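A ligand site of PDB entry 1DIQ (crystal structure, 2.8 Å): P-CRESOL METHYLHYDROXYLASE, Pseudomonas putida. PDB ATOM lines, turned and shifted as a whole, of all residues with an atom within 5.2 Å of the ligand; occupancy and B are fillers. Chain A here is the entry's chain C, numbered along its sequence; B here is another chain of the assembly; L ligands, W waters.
Water W1 lies within hydrogen-bond range of O of Phe 381 of chain B (3.1 Å) and OD1 of Asn 385 of chain B (3.3 Å).
SG of Cys 18 is bonded to C25 of the ligand, 1.9 Å away. OH of Tyr 38 sits at hydrogen-bond distance from O2 of the ligand, at 2.8 Å. The guanidinium group (NH1) of Arg 32 is in salt-bridge range of an oxygen (O1) of the ligand (3.0 Å). SD of Met 50 binds FE1 of the ligand (2.3 Å). The side-chain sulfur (SG) of Cys 15 is bonded to a carbon (C18) of the ligand (1.8 Å). An oxygen (O3) of the ligand lies within salt-bridge range of the guanidinium group of Arg 48 (3.4 Å). FE1 of the ligand is bound by NE2 of His 19, 2.1 Å away.
Val 14 touches the ligand. O of Val 25 touches C31 of the ligand (3.3 Å). CA of Gly 26 touches C28 of the ligand (3.8 Å). Pro 27 touches the ligand (CG to C11, 3.6 Å). Leu 29 touches the ligand. Ile 39 touches the ligand. CG2 of Ile 42 touches C7 of the ligand, 3.6 Å away. Val 43 touches the ligand. O of Phe 47 touches C33 of the ligand (3.3 Å). N of Ala 49 touches O4 of the ligand, at 3.8 Å. Pro 51 touches the ligand (CD to C26, 3.9 Å). Phe 53 touches the ligand. Leu 378 of chain B touches the ligand. CD1 of Phe 381 of chain B touches C26 of the ligand (3.6 Å). Hydrophobic or aromatic side chains within 4 Å of the ligand: His 19, Pro 27, Leu 29, Tyr 38, Ile 39, Ile 42, Val 43, Phe 47, Ala 49, Met 50, Pro 51, Phe 53, Leu 378 of chain B and Phe 381 of chain B. Along chain A the residues within 4 Å of the ligand span positions 14 to 53. The nearest printed residue that does not touch the ligand is Asn 385 of chain B (4.1 Å).
The backbone carbonyl oxygen (O) of Cys 18 is in hydrogen-bond range of the backbone NH (N) of Gly 26. The side-chain amide nitrogen (ND2) of Asn 385 of chain B is in hydrogen-bond range of the backbone carbonyl oxygen (O) of Val 25 (2.8 Å). N of Val 25 lies within hydrogen-bond range of O of Cys 18, 3.1 Å away. ND1 of His 19 sits at hydrogen-bond distance from O of Pro 27, 2.7 Å away. N of Phe 53 lies within hydrogen-bond range of O of Val 43, at 3.0 Å.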
ATOM      1  N   LEU A  10      11.258   5.657  -8.827  1.00  0.00           N
ATOM      2  CA  LEU A  10      10.545   6.086 -10.038  1.00  0.00           C
ATOM      3  C   LEU A  10       9.135   6.515  -9.664  1.00  0.00           C
ATOM      4  O   LEU A  10       8.685   7.576 -10.071  1.00  0.00           O
ATOM      5  CB  LEU A  10      10.485   4.981 -11.101  1.00  0.00           C
ATOM      6  CG  LEU A  10       9.654   5.251 -12.369  1.00  0.00           C
ATOM      7  CD1 LEU A  10      10.138   6.484 -13.129  1.00  0.00           C
ATOM      8  CD2 LEU A  10       9.724   4.043 -13.258  1.00  0.00           C
ATOM      9  N   VAL A  14       8.195  10.431 -10.213  1.00  0.00           N
ATOM     10  CA  VAL A  14       7.385  10.671 -11.418  1.00  0.00           C
ATOM     11  C   VAL A  14       5.921  10.250 -11.310  1.00  0.00           C
ATOM     12  O   VAL A  14       5.046  11.106 -11.201  1.00  0.00           O
ATOM     13  CB  VAL A  14       8.003  10.019 -12.686  1.00  0.00           C
ATOM     14  CG1 VAL A  14       7.163  10.348 -13.927  1.00  0.00           C
ATOM     15  CG2 VAL A  14       9.394  10.489 -12.902  1.00  0.00           C
ATOM     16  N   CYS A  15       5.679   8.925 -11.340  1.00  0.00           N
ATOM     17  CA  CYS A  15       4.328   8.353 -11.332  1.00  0.00           C
ATOM     18  C   CYS A  15       3.413   8.764 -10.196  1.00  0.00           C
ATOM     19  O   CYS A  15       2.300   9.214 -10.440  1.00  0.00           O
ATOM     20  CB  CYS A  15       4.374   6.829 -11.430  1.00  0.00           C
ATOM     21  SG  CYS A  15       5.673   6.099 -12.493  1.00  0.00           S
ATOM     22  N   CYS A  18       0.883  11.865  -9.782  1.00  0.00           N
ATOM     23  CA  CYS A  18      -0.441  11.784 -10.356  1.00  0.00           C
ATOM     24  C   CYS A  18      -1.255  10.594  -9.791  1.00  0.00           C
ATOM     25  O   CYS A  18      -2.457  10.708  -9.533  1.00  0.00           O
ATOM     26  CB  CYS A  18      -0.350  11.648 -11.873  1.00  0.00           C
ATOM     27  SG  CYS A  18       0.102  13.138 -12.825  1.00  0.00           S
ATOM     28  N   HIS A  19      -0.561   9.489  -9.507  1.00  0.00           N
ATOM     29  CA  HIS A  19      -1.173   8.250  -9.050  1.00  0.00           C
ATOM     30  C   HIS A  19      -1.386   7.945  -7.576  1.00  0.00           C
ATOM     31  O   HIS A  19      -2.163   7.054  -7.263  1.00  0.00           O
ATOM     32  CB  HIS A  19      -0.471   7.078  -9.740  1.00  0.00           C
ATOM     33  CG  HIS A  19      -0.873   6.919 -11.173  1.00  0.00           C
ATOM     34  ND1 HIS A  19      -2.143   6.543 -11.479  1.00  0.00           N
ATOM     35  CD2 HIS A  19       0.014   7.153 -12.145  1.00  0.00           C
ATOM     36  CE1 HIS A  19      -2.050   6.540 -12.860  1.00  0.00           C
ATOM     37  NE2 HIS A  19      -0.764   6.902 -13.268  1.00  0.00           N
ATOM     38  N   VAL A  25      -5.230  12.096  -9.705  1.00  0.00           N
ATOM     39  CA  VAL A  25      -5.312  12.582 -11.098  1.00  0.00           C
ATOM     40  C   VAL A  25      -5.502  11.317 -11.948  1.00  0.00           C
ATOM     41  O   VAL A  25      -6.224  11.315 -12.943  1.00  0.00           O
ATOM     42  CB  VAL A  25      -3.983  13.319 -11.526  1.00  0.00           C
ATOM     43  CG1 VAL A  25      -3.933  13.580 -13.030  1.00  0.00           C
ATOM     44  CG2 VAL A  25      -3.850  14.614 -10.788  1.00  0.00           C
ATOM     45  N   GLY A  26      -4.815  10.251 -11.518  1.00  0.00           N
ATOM     46  CA  GLY A  26      -4.910   8.967 -12.168  1.00  0.00           C
ATOM     47  C   GLY A  26      -5.378   7.924 -11.158  1.00  0.00           C
ATOM     48  O   GLY A  26      -5.352   8.193  -9.945  1.00  0.00           O
ATOM     49  N   PRO A  27      -5.825   6.746 -11.605  1.00  0.00           N
ATOM     50  CA  PRO A  27      -6.288   5.687 -10.695  1.00  0.00           C
ATOM     51  C   PRO A  27      -5.166   5.087  -9.849  1.00  0.00           C
ATOM     52  O   PRO A  27      -4.000   5.096 -10.247  1.00  0.00           O
ATOM     53  CB  PRO A  27      -6.887   4.644 -11.639  1.00  0.00           C
ATOM     54  CG  PRO A  27      -6.112   4.846 -12.905  1.00  0.00           C
ATOM     55  CD  PRO A  27      -6.066   6.346 -13.003  1.00  0.00           C
ATOM     56  N   LEU A  29      -2.660   2.581  -8.373  1.00  0.00           N
ATOM     57  CA  LEU A  29      -1.964   1.439  -8.988  1.00  0.00           C
ATOM     58  C   LEU A  29      -1.342   0.536  -7.920  1.00  0.00           C
ATOM     59  O   LEU A  29      -0.899  -0.575  -8.223  1.00  0.00           O
ATOM     60  CB  LEU A  29      -0.880   1.920  -9.951  1.00  0.00           C
ATOM     61  CG  LEU A  29      -1.156   2.888 -11.098  1.00  0.00           C
ATOM     62  CD1 LEU A  29       0.153   3.166 -11.785  1.00  0.00           C
ATOM     63  CD2 LEU A  29      -2.173   2.360 -12.073  1.00  0.00           C
ATOM     64  N   ARG A  32      -2.608  -3.548  -6.986  1.00  0.00           N
ATOM     65  CA  ARG A  32      -3.657  -3.930  -7.908  1.00  0.00           C
ATOM     66  C   ARG A  32      -3.272  -5.111  -8.799  1.00  0.00           C
ATOM     67  O   ARG A  32      -4.108  -5.648  -9.531  1.00  0.00           O
ATOM     68  CB  ARG A  32      -4.147  -2.726  -8.722  1.00  0.00           C
ATOM     69  CG  ARG A  32      -5.320  -1.987  -8.034  1.00  0.00           C
ATOM     70  CD  ARG A  32      -5.971  -0.932  -8.914  1.00  0.00           C
ATOM     71  NE  ARG A  32      -6.327  -1.395 -10.255  1.00  0.00           N
ATOM     72  CZ  ARG A  32      -6.259  -0.650 -11.370  1.00  0.00           C
ATOM     73  NH1 ARG A  32      -5.857   0.608 -11.327  1.00  0.00           N
ATOM     74  NH2 ARG A  32      -6.601  -1.175 -12.528  1.00  0.00           N
ATOM     75  N   LEU A  34      -1.176  -5.288 -11.365  1.00  0.00           N
ATOM     76  CA  LEU A  34      -1.128  -4.973 -12.788  1.00  0.00           C
ATOM     77  C   LEU A  34       0.123  -5.574 -13.464  1.00  0.00           C
ATOM     78  O   LEU A  34       1.231  -5.432 -12.954  1.00  0.00           O
ATOM     79  CB  LEU A  34      -1.175  -3.461 -13.001  1.00  0.00           C
ATOM     80  CG  LEU A  34      -2.485  -2.755 -12.664  1.00  0.00           C
ATOM     81  CD1 LEU A  34      -2.258  -1.267 -12.685  1.00  0.00           C
ATOM     82  CD2 LEU A  34      -3.541  -3.125 -13.652  1.00  0.00           C
ATOM     83  N   TYR A  38       1.569  -4.752 -19.327  1.00  0.00           N
ATOM     84  CA  TYR A  38       0.505  -3.772 -19.460  1.00  0.00           C
ATOM     85  C   TYR A  38       1.006  -2.367 -19.079  1.00  0.00           C
ATOM     86  O   TYR A  38       0.686  -1.397 -19.764  1.00  0.00           O
ATOM     87  CB  TYR A  38      -0.703  -4.162 -18.603  1.00  0.00           C
ATOM     88  CG  TYR A  38      -1.810  -3.126 -18.580  1.00  0.00           C
ATOM     89  CD1 TYR A  38      -2.487  -2.761 -19.780  1.00  0.00           C
ATOM     90  CD2 TYR A  38      -2.154  -2.470 -17.358  1.00  0.00           C
ATOM     91  CE1 TYR A  38      -3.488  -1.769 -19.769  1.00  0.00           C
ATOM     92  CE2 TYR A  38      -3.136  -1.480 -17.332  1.00  0.00           C
ATOM     93  CZ  TYR A  38      -3.809  -1.126 -18.539  1.00  0.00           C
ATOM     94  OH  TYR A  38      -4.814  -0.177 -18.487  1.00  0.00           O
ATOM     95  N   ILE A  39       1.743  -2.276 -17.966  1.00  0.00           N
ATOM     96  CA  ILE A  39       2.337  -1.029 -17.499  1.00  0.00           C
ATOM     97  C   ILE A  39       3.317  -0.476 -18.540  1.00  0.00           C
ATOM     98  O   ILE A  39       3.354   0.719 -18.777  1.00  0.00           O
ATOM     99  CB  ILE A  39       3.016  -1.247 -16.114  1.00  0.00           C
ATOM    100  CG1 ILE A  39       1.936  -1.337 -15.045  1.00  0.00           C
ATOM    101  CG2 ILE A  39       4.054  -0.159 -15.812  1.00  0.00           C
ATOM    102  CD1 ILE A  39       2.418  -1.597 -13.655  1.00  0.00           C
ATOM    103  N   ILE A  42       1.123   1.148 -21.451  1.00  0.00           N
ATOM    104  CA  ILE A  42       0.510   2.416 -21.101  1.00  0.00           C
ATOM    105  C   ILE A  42       1.547   3.533 -21.035  1.00  0.00           C
ATOM    106  O   ILE A  42       1.296   4.627 -21.519  1.00  0.00           O
ATOM    107  CB  ILE A  42      -0.291   2.324 -19.763  1.00  0.00           C
ATOM    108  CG1 ILE A  42      -1.487   1.387 -19.932  1.00  0.00           C
ATOM    109  CG2 ILE A  42      -0.812   3.665 -19.299  1.00  0.00           C
ATOM    110  CD1 ILE A  42      -2.397   1.661 -21.162  1.00  0.00           C
ATOM    111  N   VAL A  43       2.741   3.245 -20.501  1.00  0.00           N
ATOM    112  CA  VAL A  43       3.788   4.268 -20.401  1.00  0.00           C
ATOM    113  C   VAL A  43       4.402   4.577 -21.762  1.00  0.00           C
ATOM    114  O   VAL A  43       4.662   5.739 -22.066  1.00  0.00           O
ATOM    115  CB  VAL A  43       4.835   3.903 -19.342  1.00  0.00           C
ATOM    116  CG1 VAL A  43       5.957   4.920 -19.247  1.00  0.00           C
ATOM    117  CG2 VAL A  43       4.166   3.877 -18.027  1.00  0.00           C
ATOM    118  N   PHE A  47      -2.083   6.819 -22.325  1.00  0.00           N
ATOM    119  CA  PHE A  47      -3.488   6.449 -22.385  1.00  0.00           C
ATOM    120  C   PHE A  47      -4.410   7.624 -22.122  1.00  0.00           C
ATOM    121  O   PHE A  47      -4.618   8.019 -20.959  1.00  0.00           O
ATOM    122  CB  PHE A  47      -3.781   5.279 -21.439  1.00  0.00           C
ATOM    123  CG  PHE A  47      -5.180   4.747 -21.553  1.00  0.00           C
ATOM    124  CD1 PHE A  47      -5.689   4.358 -22.815  1.00  0.00           C
ATOM    125  CD2 PHE A  47      -6.016   4.728 -20.426  1.00  0.00           C
ATOM    126  CE1 PHE A  47      -7.034   3.950 -22.949  1.00  0.00           C
ATOM    127  CE2 PHE A  47      -7.374   4.321 -20.541  1.00  0.00           C
ATOM    128  CZ  PHE A  47      -7.881   3.930 -21.813  1.00  0.00           C
ATOM    129  N   ARG A  48      -5.011   8.125 -23.204  1.00  0.00           N
ATOM    130  CA  ARG A  48      -5.942   9.256 -23.203  1.00  0.00           C
ATOM    131  C   ARG A  48      -5.350  10.477 -22.490  1.00  0.00           C
ATOM    132  O   ARG A  48      -4.491  11.158 -23.051  1.00  0.00           O
ATOM    133  CB  ARG A  48      -7.288   8.888 -22.544  1.00  0.00           C
ATOM    134  CG  ARG A  48      -8.141   7.808 -23.191  1.00  0.00           C
ATOM    135  CD  ARG A  48      -9.430   7.807 -22.400  1.00  0.00           C
ATOM    136  NE  ARG A  48     -10.284   6.635 -22.577  1.00  0.00           N
ATOM    137  CZ  ARG A  48     -10.789   5.936 -21.561  1.00  0.00           C
ATOM    138  NH1 ARG A  48     -10.526   6.271 -20.300  1.00  0.00           N
ATOM    139  NH2 ARG A  48     -11.608   4.909 -21.819  1.00  0.00           N
ATOM    140  N   ALA A  49      -5.778  10.717 -21.247  1.00  0.00           N
ATOM    141  CA  ALA A  49      -5.331  11.834 -20.410  1.00  0.00           C
ATOM    142  C   ALA A  49      -3.882  11.678 -19.946  1.00  0.00           C
ATOM    143  O   ALA A  49      -3.204  12.681 -19.666  1.00  0.00           O
ATOM    144  CB  ALA A  49      -6.261  11.992 -19.217  1.00  0.00           C
ATOM    145  N   MET A  50      -3.416  10.436 -19.900  1.00  0.00           N
ATOM    146  CA  MET A  50      -2.042  10.117 -19.504  1.00  0.00           C
ATOM    147  C   MET A  50      -1.002  10.346 -20.613  1.00  0.00           C
ATOM    148  O   MET A  50      -1.181   9.905 -21.751  1.00  0.00           O
ATOM    149  CB  MET A  50      -1.892   8.655 -19.044  1.00  0.00           C
ATOM    150  CG  MET A  50      -0.487   8.408 -18.451  1.00  0.00           C
ATOM    151  SD  MET A  50      -0.049   6.995 -17.545  1.00  0.00           S
ATOM    152  CE  MET A  50       1.524   6.720 -18.220  1.00  0.00           C
ATOM    153  N   PRO A  51       0.100  11.036 -20.266  1.00  0.00           N
ATOM    154  CA  PRO A  51       1.141  11.260 -21.281  1.00  0.00           C
ATOM    155  C   PRO A  51       1.996   9.992 -21.482  1.00  0.00           C
ATOM    156  O   PRO A  51       1.908   9.039 -20.718  1.00  0.00           O
ATOM    157  CB  PRO A  51       1.978  12.365 -20.642  1.00  0.00           C
ATOM    158  CG  PRO A  51       1.785  12.190 -19.174  1.00  0.00           C
ATOM    159  CD  PRO A  51       0.307  11.925 -19.105  1.00  0.00           C
ATOM    160  N   PHE A  53       5.889   8.426 -21.964  1.00  0.00           N
ATOM    161  CA  PHE A  53       7.259   8.753 -21.608  1.00  0.00           C
ATOM    162  C   PHE A  53       8.196   7.916 -22.461  1.00  0.00           C
ATOM    163  O   PHE A  53       8.030   6.690 -22.543  1.00  0.00           O
ATOM    164  CB  PHE A  53       7.544   8.458 -20.150  1.00  0.00           C
ATOM    165  CG  PHE A  53       6.775   9.284 -19.202  1.00  0.00           C
ATOM    166  CD1 PHE A  53       5.475   8.903 -18.812  1.00  0.00           C
ATOM    167  CD2 PHE A  53       7.343  10.425 -18.641  1.00  0.00           C
ATOM    168  CE1 PHE A  53       4.754   9.664 -17.871  1.00  0.00           C
ATOM    169  CE2 PHE A  53       6.637  11.202 -17.690  1.00  0.00           C
ATOM    170  CZ  PHE A  53       5.341  10.809 -17.308  1.00  0.00           C
ATOM    171  N   VAL A  58      12.191   7.309 -19.041  1.00  0.00           N
ATOM    172  CA  VAL A  58      11.967   6.145 -18.167  1.00  0.00           C
ATOM    173  C   VAL A  58      12.269   4.903 -19.017  1.00  0.00           C
ATOM    174  O   VAL A  58      11.491   4.594 -19.928  1.00  0.00           O
ATOM    175  CB  VAL A  58      10.472   6.063 -17.654  1.00  0.00           C
ATOM    176  CG1 VAL A  58      10.301   4.936 -16.686  1.00  0.00           C
ATOM    177  CG2 VAL A  58      10.039   7.325 -16.969  1.00  0.00           C
ATOM    178  N   LEU A  63      10.833   0.309 -15.737  1.00  0.00           N
ATOM    179  CA  LEU A  63       9.418  -0.042 -15.835  1.00  0.00           C
ATOM    180  C   LEU A  63       9.178  -1.387 -15.140  1.00  0.00           C
ATOM    181  O   LEU A  63       8.170  -1.552 -14.437  1.00  0.00           O
ATOM    182  CB  LEU A  63       8.972  -0.092 -17.302  1.00  0.00           C
ATOM    183  CG  LEU A  63       8.702   1.272 -17.947  1.00  0.00           C
ATOM    184  CD1 LEU A  63       8.382   1.098 -19.424  1.00  0.00           C
ATOM    185  CD2 LEU A  63       7.559   1.996 -17.219  1.00  0.00           C
ATOM    186  N   VAL A  66       9.265  -0.769 -11.348  1.00  0.00           N
ATOM    187  CA  VAL A  66       8.058  -0.106 -10.826  1.00  0.00           C
ATOM    188  C   VAL A  66       6.835  -1.028 -10.805  1.00  0.00           C
ATOM    189  O   VAL A  66       5.999  -0.947  -9.889  1.00  0.00           O
ATOM    190  CB  VAL A  66       7.766   1.284 -11.512  1.00  0.00           C
ATOM    191  CG1 VAL A  66       7.115   1.139 -12.889  1.00  0.00           C
ATOM    192  CG2 VAL A  66       6.936   2.189 -10.573  1.00  0.00           C
ATOM    193  N   ILE B 158       8.085  16.938 -13.746  1.00  0.00           N
ATOM    194  CA  ILE B 158       8.415  16.262 -14.987  1.00  0.00           C
ATOM    195  C   ILE B 158       8.979  17.139 -16.097  1.00  0.00           C
ATOM    196  O   ILE B 158       9.586  16.613 -17.020  1.00  0.00           O
ATOM    197  CB  ILE B 158       7.235  15.388 -15.513  1.00  0.00           C
ATOM    198  CG1 ILE B 158       5.981  16.238 -15.774  1.00  0.00           C
ATOM    199  CG2 ILE B 158       6.964  14.234 -14.524  1.00  0.00           C
ATOM    200  CD1 ILE B 158       4.852  15.507 -16.512  1.00  0.00           C
ATOM    201  N   LEU B 378       1.746  17.767  -9.469  1.00  0.00           N
ATOM    202  CA  LEU B 378       1.123  17.646 -10.784  1.00  0.00           C
ATOM    203  C   LEU B 378      -0.403  17.677 -10.679  1.00  0.00           C
ATOM    204  O   LEU B 378      -1.119  17.237 -11.580  1.00  0.00           O
ATOM    205  CB  LEU B 378       1.603  16.370 -11.479  1.00  0.00           C
ATOM    206  CG  LEU B 378       2.742  16.524 -12.479  1.00  0.00           C
ATOM    207  CD1 LEU B 378       3.998  17.044 -11.835  1.00  0.00           C
ATOM    208  CD2 LEU B 378       3.008  15.170 -13.131  1.00  0.00           C
ATOM    209  N   PHE B 381      -3.150  18.682 -13.395  1.00  0.00           N
ATOM    210  CA  PHE B 381      -3.461  17.766 -14.496  1.00  0.00           C
ATOM    211  C   PHE B 381      -4.886  17.214 -14.433  1.00  0.00           C
ATOM    212  O   PHE B 381      -5.357  16.514 -15.352  1.00  0.00           O
ATOM    213  CB  PHE B 381      -2.433  16.649 -14.556  1.00  0.00           C
ATOM    214  CG  PHE B 381      -1.222  16.996 -15.340  1.00  0.00           C
ATOM    215  CD1 PHE B 381      -1.052  16.489 -16.649  1.00  0.00           C
ATOM    216  CD2 PHE B 381      -0.230  17.823 -14.795  1.00  0.00           C
ATOM    217  CE1 PHE B 381       0.088  16.816 -17.409  1.00  0.00           C
ATOM    218  CE2 PHE B 381       0.917  18.154 -15.544  1.00  0.00           C
ATOM    219  CZ  PHE B 381       1.076  17.655 -16.858  1.00  0.00           C
ATOM    220  N   ASN B 385      -9.209  15.704 -16.770  1.00  0.00           N
ATOM    221  CA  ASN B 385     -10.207  14.781 -16.281  1.00  0.00           C
ATOM    222  C   ASN B 385     -11.581  15.416 -16.304  1.00  0.00           C
ATOM    223  O   ASN B 385     -12.571  14.708 -16.156  1.00  0.00           O
ATOM    224  CB  ASN B 385      -9.874  14.281 -14.870  1.00  0.00           C
ATOM    225  CG  ASN B 385      -8.642  13.384 -14.842  1.00  0.00           C
ATOM    226  OD1 ASN B 385      -8.248  12.804 -15.864  1.00  0.00           O
ATOM    227  ND2 ASN B 385      -8.026  13.272 -13.671  1.00  0.00           N
HETATM  228 FE1  LIG L   1      -0.398   6.995 -15.322  1.00  0.00          FE
HETATM  229  C1  LIG L   1      -3.467   5.729 -16.063  1.00  0.00           C
HETATM  230  C2  LIG L   1       0.930   3.854 -15.232  1.00  0.00           C
HETATM  231  C3  LIG L   1       2.715   8.286 -14.643  1.00  0.00           C
HETATM  232  C4  LIG L   1      -1.679  10.134 -15.268  1.00  0.00           C
HETATM  233  N1  LIG L   1      -1.136   5.130 -15.605  1.00  0.00           N
HETATM  234  C5  LIG L   1      -2.436   4.824 -15.902  1.00  0.00           C
HETATM  235  C6  LIG L   1      -2.553   3.376 -16.016  1.00  0.00           C
HETATM  236  C7  LIG L   1      -1.323   2.843 -15.782  1.00  0.00           C
HETATM  237  C8  LIG L   1      -0.418   3.941 -15.527  1.00  0.00           C
HETATM  238  C9  LIG L   1      -0.908   1.366 -15.773  1.00  0.00           C
HETATM  239  C10 LIG L   1      -3.868   2.648 -16.329  1.00  0.00           C
HETATM  240  C11 LIG L   1      -4.606   2.327 -15.029  1.00  0.00           C
HETATM  241  C12 LIG L   1      -5.878   1.531 -15.203  1.00  0.00           C
HETATM  242  O1  LIG L   1      -6.575   1.357 -14.129  1.00  0.00           O
HETATM  243  O2  LIG L   1      -6.151   1.084 -16.325  1.00  0.00           O
HETATM  244  N2  LIG L   1       1.448   6.241 -14.998  1.00  0.00           N
HETATM  245  C13 LIG L   1       1.792   4.887 -14.990  1.00  0.00           C
HETATM  246  C14 LIG L   1       3.196   4.731 -14.679  1.00  0.00           C
HETATM  247  C15 LIG L   1       3.699   5.990 -14.523  1.00  0.00           C
HETATM  248  C16 LIG L   1       2.624   6.918 -14.719  1.00  0.00           C
HETATM  249  C17 LIG L   1       3.936   3.399 -14.562  1.00  0.00           C
HETATM  250  C18 LIG L   1       5.146   6.433 -14.192  1.00  0.00           C
HETATM  251  C19 LIG L   1       6.177   6.018 -15.243  1.00  0.00           C
HETATM  252  N3  LIG L   1       0.349   8.830 -15.041  1.00  0.00           N
HETATM  253  C20 LIG L   1       1.675   9.167 -14.768  1.00  0.00           C
HETATM  254  C21 LIG L   1       1.818  10.606 -14.595  1.00  0.00           C
HETATM  255  C22 LIG L   1       0.580  11.131 -14.734  1.00  0.00           C
HETATM  256  C23 LIG L   1      -0.331  10.030 -15.032  1.00  0.00           C
HETATM  257  C24 LIG L   1       3.160  11.308 -14.281  1.00  0.00           C
HETATM  258  C25 LIG L   1       0.129  12.597 -14.601  1.00  0.00           C
HETATM  259  C26 LIG L   1       0.784  13.585 -15.575  1.00  0.00           C
HETATM  260  N4  LIG L   1      -2.189   7.769 -15.620  1.00  0.00           N
HETATM  261  C27 LIG L   1      -2.551   9.120 -15.548  1.00  0.00           C
HETATM  262  C28 LIG L   1      -3.969   9.271 -15.828  1.00  0.00           C
HETATM  263  C29 LIG L   1      -4.464   8.022 -16.069  1.00  0.00           C
HETATM  264  C30 LIG L   1      -3.373   7.094 -15.923  1.00  0.00           C
HETATM  265  C31 LIG L   1      -4.751  10.607 -15.860  1.00  0.00           C
HETATM  266  C32 LIG L   1      -5.909   7.701 -16.419  1.00  0.00           C
HETATM  267  C33 LIG L   1      -6.070   7.824 -17.949  1.00  0.00           C
HETATM  268  C34 LIG L   1      -7.465   7.546 -18.373  1.00  0.00           C
HETATM  269  O3  LIG L   1      -8.027   6.483 -18.012  1.00  0.00           O
HETATM  270  O4  LIG L   1      -7.972   8.446 -19.086  1.00  0.00           O
HETATM  271  O   HOH W   1      -5.041  13.503 -16.206  1.00  0.00           O
HETATM  272  O   HOH W   2      -9.054   2.172 -12.932  1.00  0.00           O
